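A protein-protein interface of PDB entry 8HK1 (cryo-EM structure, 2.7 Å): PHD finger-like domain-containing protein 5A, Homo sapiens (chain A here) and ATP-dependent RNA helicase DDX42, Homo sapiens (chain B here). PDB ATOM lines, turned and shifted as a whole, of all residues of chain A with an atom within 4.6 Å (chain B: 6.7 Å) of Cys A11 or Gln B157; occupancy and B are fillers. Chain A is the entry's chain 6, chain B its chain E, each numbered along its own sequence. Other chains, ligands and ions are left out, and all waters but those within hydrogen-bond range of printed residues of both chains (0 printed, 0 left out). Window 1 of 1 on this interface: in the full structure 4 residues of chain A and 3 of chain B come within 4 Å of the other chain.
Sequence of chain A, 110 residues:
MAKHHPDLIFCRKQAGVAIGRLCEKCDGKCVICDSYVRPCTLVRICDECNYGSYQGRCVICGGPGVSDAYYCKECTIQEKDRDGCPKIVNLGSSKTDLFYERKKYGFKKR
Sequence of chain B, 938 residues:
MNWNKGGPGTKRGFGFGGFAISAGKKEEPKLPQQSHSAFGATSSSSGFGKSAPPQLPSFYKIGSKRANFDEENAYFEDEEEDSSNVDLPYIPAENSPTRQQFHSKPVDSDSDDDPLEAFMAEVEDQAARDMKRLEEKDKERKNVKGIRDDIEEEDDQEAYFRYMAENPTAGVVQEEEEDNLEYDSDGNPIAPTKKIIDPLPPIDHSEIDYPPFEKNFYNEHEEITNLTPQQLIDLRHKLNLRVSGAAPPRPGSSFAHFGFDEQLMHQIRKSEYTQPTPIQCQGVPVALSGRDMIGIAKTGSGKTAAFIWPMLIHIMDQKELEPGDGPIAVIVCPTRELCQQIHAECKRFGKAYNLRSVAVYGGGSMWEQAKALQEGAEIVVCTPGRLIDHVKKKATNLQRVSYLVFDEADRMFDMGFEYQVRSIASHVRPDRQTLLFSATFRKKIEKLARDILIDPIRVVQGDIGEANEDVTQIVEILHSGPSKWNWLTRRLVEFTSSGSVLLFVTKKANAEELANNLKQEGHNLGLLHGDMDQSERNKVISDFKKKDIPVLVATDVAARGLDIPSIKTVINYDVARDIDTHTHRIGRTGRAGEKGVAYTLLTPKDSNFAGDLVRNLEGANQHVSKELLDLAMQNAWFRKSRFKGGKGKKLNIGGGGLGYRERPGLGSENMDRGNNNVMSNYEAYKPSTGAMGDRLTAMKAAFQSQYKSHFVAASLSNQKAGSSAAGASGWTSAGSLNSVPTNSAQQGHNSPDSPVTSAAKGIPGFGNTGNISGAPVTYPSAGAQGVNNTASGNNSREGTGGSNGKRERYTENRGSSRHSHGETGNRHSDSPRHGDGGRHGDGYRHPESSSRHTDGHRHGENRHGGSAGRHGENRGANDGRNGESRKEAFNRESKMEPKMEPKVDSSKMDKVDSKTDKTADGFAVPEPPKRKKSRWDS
Of the printed residues of chain B, Ile A9 touches Tyr B160 (3.7 Å). Of the printed residues of chain B, Cys A11 touches Gln B157 (3.6 Å). Printed residues of chain B within 4 Å of Lys A13: Gln B157 (2.8 Å). Gln B157 touches just these residues of chain A: Cys A11 (3.6 Å) and Lys A13 (2.8 Å). Of the printed residues of chain A, Tyr B160 touches Ile A9 (3.7 Å). The nearest residue of chain A that does not touch Gln B157 is Val A89 (4.5 Å).
The backbone carbonyl oxygen of Ile A9 lies within hydrogen-bond range of the backbone NH of Val A89 (2.9 Å). N of Cys A11 lies within hydrogen-bond range of O of Lys A87, at 3.0 Å. The backbone carbonyl oxygen of Lys A13 lies within hydrogen-bond range of the backbone NH of Cys A85 (2.7 Å).
The side-chain amino group (NZ) of Lys A13 lies close to the side-chain amide nitrogen (NE2) of Gln B157, at 2.8 Å.
Of the 9 printed residues of chain B, 2 touch a printed residue of chain A. Hydrophobic or aromatic side chains of chain B that line the printed part of chain A: Tyr B160. Hydrophobic or aromatic side chains of chain A within 4 Å of the printed part of chain B: Ile A9. Among the printed residues, no Asp or Glu carboxylate lies within 4 Å of a Lys or Arg side-chain nitrogen of the other chain.
Tyr B160 touches Ile A9. NE2 of Gln B157 touches O of Cys A11, at 3.6 Å.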
ATOM      1  N   ILE A   9     -16.202 -34.279 -20.692  1.00  0.00           N
ATOM      2  CA  ILE A   9     -17.320 -33.503 -21.211  1.00  0.00           C
ATOM      3  C   ILE A   9     -17.980 -34.307 -22.321  1.00  0.00           C
ATOM      4  O   ILE A   9     -17.307 -34.960 -23.123  1.00  0.00           O
ATOM      5  CB  ILE A   9     -16.847 -32.118 -21.720  1.00  0.00           C
ATOM      6  CG1 ILE A   9     -16.308 -31.278 -20.557  1.00  0.00           C
ATOM      7  CG2 ILE A   9     -17.968 -31.392 -22.445  1.00  0.00           C
ATOM      8  CD1 ILE A   9     -17.305 -30.303 -19.974  1.00  0.00           C
ATOM      9  N   PHE A  10     -19.309 -34.266 -22.358  1.00  0.00           N
ATOM     10  CA  PHE A  10     -20.051 -34.909 -23.427  1.00  0.00           C
ATOM     11  C   PHE A  10     -19.955 -34.090 -24.712  1.00  0.00           C
ATOM     12  O   PHE A  10     -19.733 -32.878 -24.684  1.00  0.00           O
ATOM     13  CB  PHE A  10     -21.513 -35.087 -23.024  1.00  0.00           C
ATOM     14  CG  PHE A  10     -21.713 -36.029 -21.870  1.00  0.00           C
ATOM     15  CD1 PHE A  10     -21.451 -37.378 -22.008  1.00  0.00           C
ATOM     16  CD2 PHE A  10     -22.151 -35.559 -20.646  1.00  0.00           C
ATOM     17  CE1 PHE A  10     -21.639 -38.243 -20.950  1.00  0.00           C
ATOM     18  CE2 PHE A  10     -22.335 -36.421 -19.588  1.00  0.00           C
ATOM     19  CZ  PHE A  10     -22.076 -37.764 -19.741  1.00  0.00           C
ATOM     20  N   CYS A  11     -20.123 -34.765 -25.849  1.00  0.00           N
ATOM     21  CA  CYS A  11     -20.030 -34.081 -27.137  1.00  0.00           C
ATOM     22  C   CYS A  11     -21.216 -33.144 -27.357  1.00  0.00           C
ATOM     23  O   CYS A  11     -21.030 -31.954 -27.633  1.00  0.00           O
ATOM     24  CB  CYS A  11     -19.926 -35.104 -28.267  1.00  0.00           C
ATOM     25  SG  CYS A  11     -19.943 -34.386 -29.921  1.00  0.00           S
ATOM     26  N   ARG A  12     -22.438 -33.672 -27.255  1.00  0.00           N
ATOM     27  CA  ARG A  12     -23.672 -32.884 -27.263  1.00  0.00           C
ATOM     28  C   ARG A  12     -23.927 -32.236 -28.627  1.00  0.00           C
ATOM     29  O   ARG A  12     -24.467 -31.134 -28.732  1.00  0.00           O
ATOM     30  CB  ARG A  12     -23.661 -31.834 -26.147  1.00  0.00           C
ATOM     31  CG  ARG A  12     -23.688 -32.410 -24.746  1.00  0.00           C
ATOM     32  CD  ARG A  12     -24.682 -33.549 -24.632  1.00  0.00           C
ATOM     33  NE  ARG A  12     -24.987 -33.865 -23.241  1.00  0.00           N
ATOM     34  CZ  ARG A  12     -25.511 -35.015 -22.834  1.00  0.00           C
ATOM     35  NH1 ARG A  12     -25.788 -35.968 -23.714  1.00  0.00           N
ATOM     36  NH2 ARG A  12     -25.754 -35.216 -21.547  1.00  0.00           N
ATOM     37  N   LYS A  13     -23.540 -32.948 -29.681  1.00  0.00           N
ATOM     38  CA  LYS A  13     -23.842 -32.551 -31.049  1.00  0.00           C
ATOM     39  C   LYS A  13     -25.068 -33.319 -31.526  1.00  0.00           C
ATOM     40  O   LYS A  13     -25.468 -34.317 -30.924  1.00  0.00           O
ATOM     41  CB  LYS A  13     -22.651 -32.801 -31.981  1.00  0.00           C
ATOM     42  CG  LYS A  13     -21.552 -31.767 -31.876  1.00  0.00           C
ATOM     43  CD  LYS A  13     -20.417 -32.085 -32.836  1.00  0.00           C
ATOM     44  CE  LYS A  13     -19.335 -31.023 -32.779  1.00  0.00           C
ATOM     45  NZ  LYS A  13     -18.747 -30.908 -31.418  1.00  0.00           N
ATOM     46  N   CYS A  46     -23.085 -38.772 -33.159  1.00  0.00           N
ATOM     47  CA  CYS A  46     -23.003 -37.879 -34.302  1.00  0.00           C
ATOM     48  C   CYS A  46     -22.043 -38.438 -35.351  1.00  0.00           C
ATOM     49  O   CYS A  46     -21.420 -39.488 -35.176  1.00  0.00           O
ATOM     50  CB  CYS A  46     -22.583 -36.483 -33.846  1.00  0.00           C
ATOM     51  SG  CYS A  46     -20.890 -36.360 -33.243  1.00  0.00           S
ATOM     52  N   GLU A  48     -19.231 -36.886 -36.609  1.00  0.00           N
ATOM     53  CA  GLU A  48     -17.807 -36.646 -36.398  1.00  0.00           C
ATOM     54  C   GLU A  48     -17.229 -37.629 -35.389  1.00  0.00           C
ATOM     55  O   GLU A  48     -16.017 -37.877 -35.386  1.00  0.00           O
ATOM     56  CB  GLU A  48     -17.562 -35.198 -35.964  1.00  0.00           C
ATOM     57  CG  GLU A  48     -18.025 -34.843 -34.557  1.00  0.00           C
ATOM     58  CD  GLU A  48     -16.902 -34.902 -33.531  1.00  0.00           C
ATOM     59  OE1 GLU A  48     -17.102 -35.514 -32.463  1.00  0.00           O
ATOM     60  OE2 GLU A  48     -15.823 -34.331 -33.789  1.00  0.00           O
ATOM     61  N   CYS A  49     -18.074 -38.200 -34.529  1.00  0.00           N
ATOM     62  CA  CYS A  49     -17.640 -39.266 -33.636  1.00  0.00           C
ATOM     63  C   CYS A  49     -17.563 -40.616 -34.335  1.00  0.00           C
ATOM     64  O   CYS A  49     -16.915 -41.532 -33.818  1.00  0.00           O
ATOM     65  CB  CYS A  49     -18.585 -39.369 -32.434  1.00  0.00           C
ATOM     66  SG  CYS A  49     -18.446 -38.024 -31.234  1.00  0.00           S
ATOM     67  N   CYS A  85     -24.968 -35.863 -28.793  1.00  0.00           N
ATOM     68  CA  CYS A  85     -24.107 -37.039 -28.777  1.00  0.00           C
ATOM     69  C   CYS A  85     -23.516 -37.226 -27.384  1.00  0.00           C
ATOM     70  O   CYS A  85     -22.915 -36.294 -26.840  1.00  0.00           O
ATOM     71  CB  CYS A  85     -23.001 -36.891 -29.818  1.00  0.00           C
ATOM     72  SG  CYS A  85     -21.846 -38.275 -29.915  1.00  0.00           S
ATOM     73  N   LYS A  87     -20.961 -39.050 -26.455  1.00  0.00           N
ATOM     74  CA  LYS A  87     -19.581 -39.524 -26.458  1.00  0.00           C
ATOM     75  C   LYS A  87     -18.733 -38.682 -25.513  1.00  0.00           C
ATOM     76  O   LYS A  87     -18.776 -37.450 -25.561  1.00  0.00           O
ATOM     77  CB  LYS A  87     -19.014 -39.475 -27.871  1.00  0.00           C
ATOM     78  CG  LYS A  87     -18.080 -40.612 -28.194  1.00  0.00           C
ATOM     79  CD  LYS A  87     -16.643 -40.135 -28.204  1.00  0.00           C
ATOM     80  CE  LYS A  87     -15.760 -41.051 -29.030  1.00  0.00           C
ATOM     81  NZ  LYS A  87     -14.323 -40.785 -28.759  1.00  0.00           N
ATOM     82  N   VAL A  89     -15.651 -36.841 -24.648  1.00  0.00           N
ATOM     83  CA  VAL A  89     -14.569 -36.228 -25.406  1.00  0.00           C
ATOM     84  C   VAL A  89     -13.670 -35.462 -24.444  1.00  0.00           C
ATOM     85  O   VAL A  89     -14.155 -34.792 -23.525  1.00  0.00           O
ATOM     86  CB  VAL A  89     -15.107 -35.316 -26.533  1.00  0.00           C
ATOM     87  CG1 VAL A  89     -16.016 -36.104 -27.465  1.00  0.00           C
ATOM     88  CG2 VAL A  89     -15.861 -34.122 -25.967  1.00  0.00           C
ATOM     89  N   GLU B 154     -20.065 -19.527 -34.954  1.00  0.00           N
ATOM     90  CA  GLU B 154     -19.374 -20.363 -33.936  1.00  0.00           C
ATOM     91  C   GLU B 154     -20.267 -21.533 -33.514  1.00  0.00           C
ATOM     92  O   GLU B 154     -21.472 -21.317 -33.299  1.00  0.00           O
ATOM     93  CB  GLU B 154     -19.065 -19.519 -32.697  1.00  0.00           C
ATOM     94  CG  GLU B 154     -17.755 -18.763 -32.783  1.00  0.00           C
ATOM     95  CD  GLU B 154     -17.362 -18.060 -31.495  1.00  0.00           C
ATOM     96  OE1 GLU B 154     -18.201 -18.006 -30.574  1.00  0.00           O
ATOM     97  OE2 GLU B 154     -16.219 -17.569 -31.416  1.00  0.00           O
ATOM     98  N   ASP B 155     -19.649 -22.698 -33.278  1.00  0.00           N
ATOM     99  CA  ASP B 155     -20.364 -23.923 -32.828  1.00  0.00           C
ATOM    100  C   ASP B 155     -20.567 -23.859 -31.307  1.00  0.00           C
ATOM    101  O   ASP B 155     -19.956 -22.984 -30.662  1.00  0.00           O
ATOM    102  CB  ASP B 155     -19.582 -25.188 -33.186  1.00  0.00           C
ATOM    103  CG  ASP B 155     -18.521 -24.975 -34.253  1.00  0.00           C
ATOM    104  OD1 ASP B 155     -18.468 -23.864 -34.816  1.00  0.00           O
ATOM    105  OD2 ASP B 155     -17.750 -25.923 -34.504  1.00  0.00           O
ATOM    106  N   ASP B 156     -21.371 -24.772 -30.756  1.00  0.00           N
ATOM    107  CA  ASP B 156     -21.646 -24.783 -29.295  1.00  0.00           C
ATOM    108  C   ASP B 156     -20.337 -25.021 -28.535  1.00  0.00           C
ATOM    109  O   ASP B 156     -20.098 -24.317 -27.535  1.00  0.00           O
ATOM    110  CB  ASP B 156     -22.655 -25.876 -28.939  1.00  0.00           C
ATOM    111  CG  ASP B 156     -23.563 -26.254 -30.093  1.00  0.00           C
ATOM    112  OD1 ASP B 156     -23.562 -25.521 -31.103  1.00  0.00           O
ATOM    113  OD2 ASP B 156     -24.264 -27.280 -29.974  1.00  0.00           O
ATOM    114  N   GLN B 157     -19.511 -25.953 -29.020  1.00  0.00           N
ATOM    115  CA  GLN B 157     -18.214 -26.263 -28.363  1.00  0.00           C
ATOM    116  C   GLN B 157     -17.314 -25.022 -28.410  1.00  0.00           C
ATOM    117  O   GLN B 157     -16.688 -24.712 -27.378  1.00  0.00           O
ATOM    118  CB  GLN B 157     -17.545 -27.458 -29.043  1.00  0.00           C
ATOM    119  CG  GLN B 157     -18.099 -28.803 -28.596  1.00  0.00           C
ATOM    120  CD  GLN B 157     -17.212 -29.946 -29.024  1.00  0.00           C
ATOM    121  OE1 GLN B 157     -16.118 -29.745 -29.544  1.00  0.00           O
ATOM    122  NE2 GLN B 157     -17.682 -31.163 -28.803  1.00  0.00           N
ATOM    123  N   GLU B 158     -17.287 -24.323 -29.548  1.00  0.00           N
ATOM    124  CA  GLU B 158     -16.449 -23.100 -29.680  1.00  0.00           C
ATOM    125  C   GLU B 158     -16.945 -22.053 -28.679  1.00  0.00           C
ATOM    126  O   GLU B 158     -16.102 -21.423 -28.017  1.00  0.00           O
ATOM    127  CB  GLU B 158     -16.513 -22.552 -31.107  1.00  0.00           C
ATOM    128  CG  GLU B 158     -15.520 -23.205 -32.049  1.00  0.00           C
ATOM    129  CD  GLU B 158     -15.333 -22.486 -33.374  1.00  0.00           C
ATOM    130  OE1 GLU B 158     -15.968 -21.431 -33.570  1.00  0.00           O
ATOM    131  OE2 GLU B 158     -14.551 -22.983 -34.209  1.00  0.00           O
ATOM    132  N   ALA B 159     -18.269 -21.916 -28.549  1.00  0.00           N
ATOM    133  CA  ALA B 159     -18.858 -20.935 -27.611  1.00  0.00           C
ATOM    134  C   ALA B 159     -18.440 -21.296 -26.183  1.00  0.00           C
ATOM    135  O   ALA B 159     -18.045 -20.385 -25.436  1.00  0.00           O
ATOM    136  CB  ALA B 159     -20.359 -20.940 -27.761  1.00  0.00           C
ATOM    137  N   TYR B 160     -18.476 -22.589 -25.846  1.00  0.00           N
ATOM    138  CA  TYR B 160     -18.085 -23.047 -24.487  1.00  0.00           C
ATOM    139  C   TYR B 160     -16.609 -22.721 -24.240  1.00  0.00           C
ATOM    140  O   TYR B 160     -16.278 -22.230 -23.143  1.00  0.00           O
ATOM    141  CB  TYR B 160     -18.336 -24.550 -24.337  1.00  0.00           C
ATOM    142  CG  TYR B 160     -17.833 -25.136 -23.042  1.00  0.00           C
ATOM    143  CD1 TYR B 160     -16.787 -26.042 -23.028  1.00  0.00           C
ATOM    144  CD2 TYR B 160     -18.391 -24.774 -21.829  1.00  0.00           C
ATOM    145  CE1 TYR B 160     -16.315 -26.582 -21.844  1.00  0.00           C
ATOM    146  CE2 TYR B 160     -17.931 -25.305 -20.635  1.00  0.00           C
ATOM    147  CZ  TYR B 160     -16.888 -26.213 -20.642  1.00  0.00           C
ATOM    148  OH  TYR B 160     -16.428 -26.739 -19.469  1.00  0.00           O
ATOM    149  N   PHE B 161     -15.756 -22.953 -25.243  1.00  0.00           N
ATOM    150  CA  PHE B 161     -14.305 -22.666 -25.091  1.00  0.00           C
ATOM    151  C   PHE B 161     -14.116 -21.162 -24.865  1.00  0.00           C
ATOM    152  O   PHE B 161     -13.340 -20.772 -23.967  1.00  0.00           O
ATOM    153  CB  PHE B 161     -13.529 -23.150 -26.318  1.00  0.00           C
ATOM    154  CG  PHE B 161     -13.538 -24.644 -26.523  1.00  0.00           C
ATOM    155  CD1 PHE B 161     -13.527 -25.509 -25.443  1.00  0.00           C
ATOM    156  CD2 PHE B 161     -13.535 -25.185 -27.799  1.00  0.00           C
ATOM    157  CE1 PHE B 161     -13.533 -26.882 -25.632  1.00  0.00           C
ATOM    158  CE2 PHE B 161     -13.539 -26.558 -27.988  1.00  0.00           C
ATOM    159  CZ  PHE B 161     -13.537 -27.404 -26.905  1.00  0.00           C
ATOM    160  N   ARG B 162     -14.862 -20.350 -25.618  1.00  0.00           N
ATOM    161  CA  ARG B 162     -14.766 -18.872 -25.495  1.00  0.00           C
ATOM    162  C   ARG B 162     -15.178 -18.476 -24.075  1.00  0.00           C
ATOM    163  O   ARG B 162     -14.459 -17.673 -23.457  1.00  0.00           O
ATOM    164  CB  ARG B 162     -15.707 -18.215 -26.508  1.00  0.00           C
ATOM    165  CG  ARG B 162     -15.244 -18.320 -27.954  1.00  0.00           C
ATOM    166  CD  ARG B 162     -14.887 -16.968 -28.538  1.00  0.00           C
ATOM    167  NE  ARG B 162     -16.077 -16.240 -28.957  1.00  0.00           N
ATOM    168  CZ  ARG B 162     -16.930 -15.649 -28.129  1.00  0.00           C
ATOM    169  NH1 ARG B 162     -16.729 -15.703 -26.823  1.00  0.00           N
ATOM    170  NH2 ARG B 162     -17.981 -15.011 -28.607  1.00  0.00           N
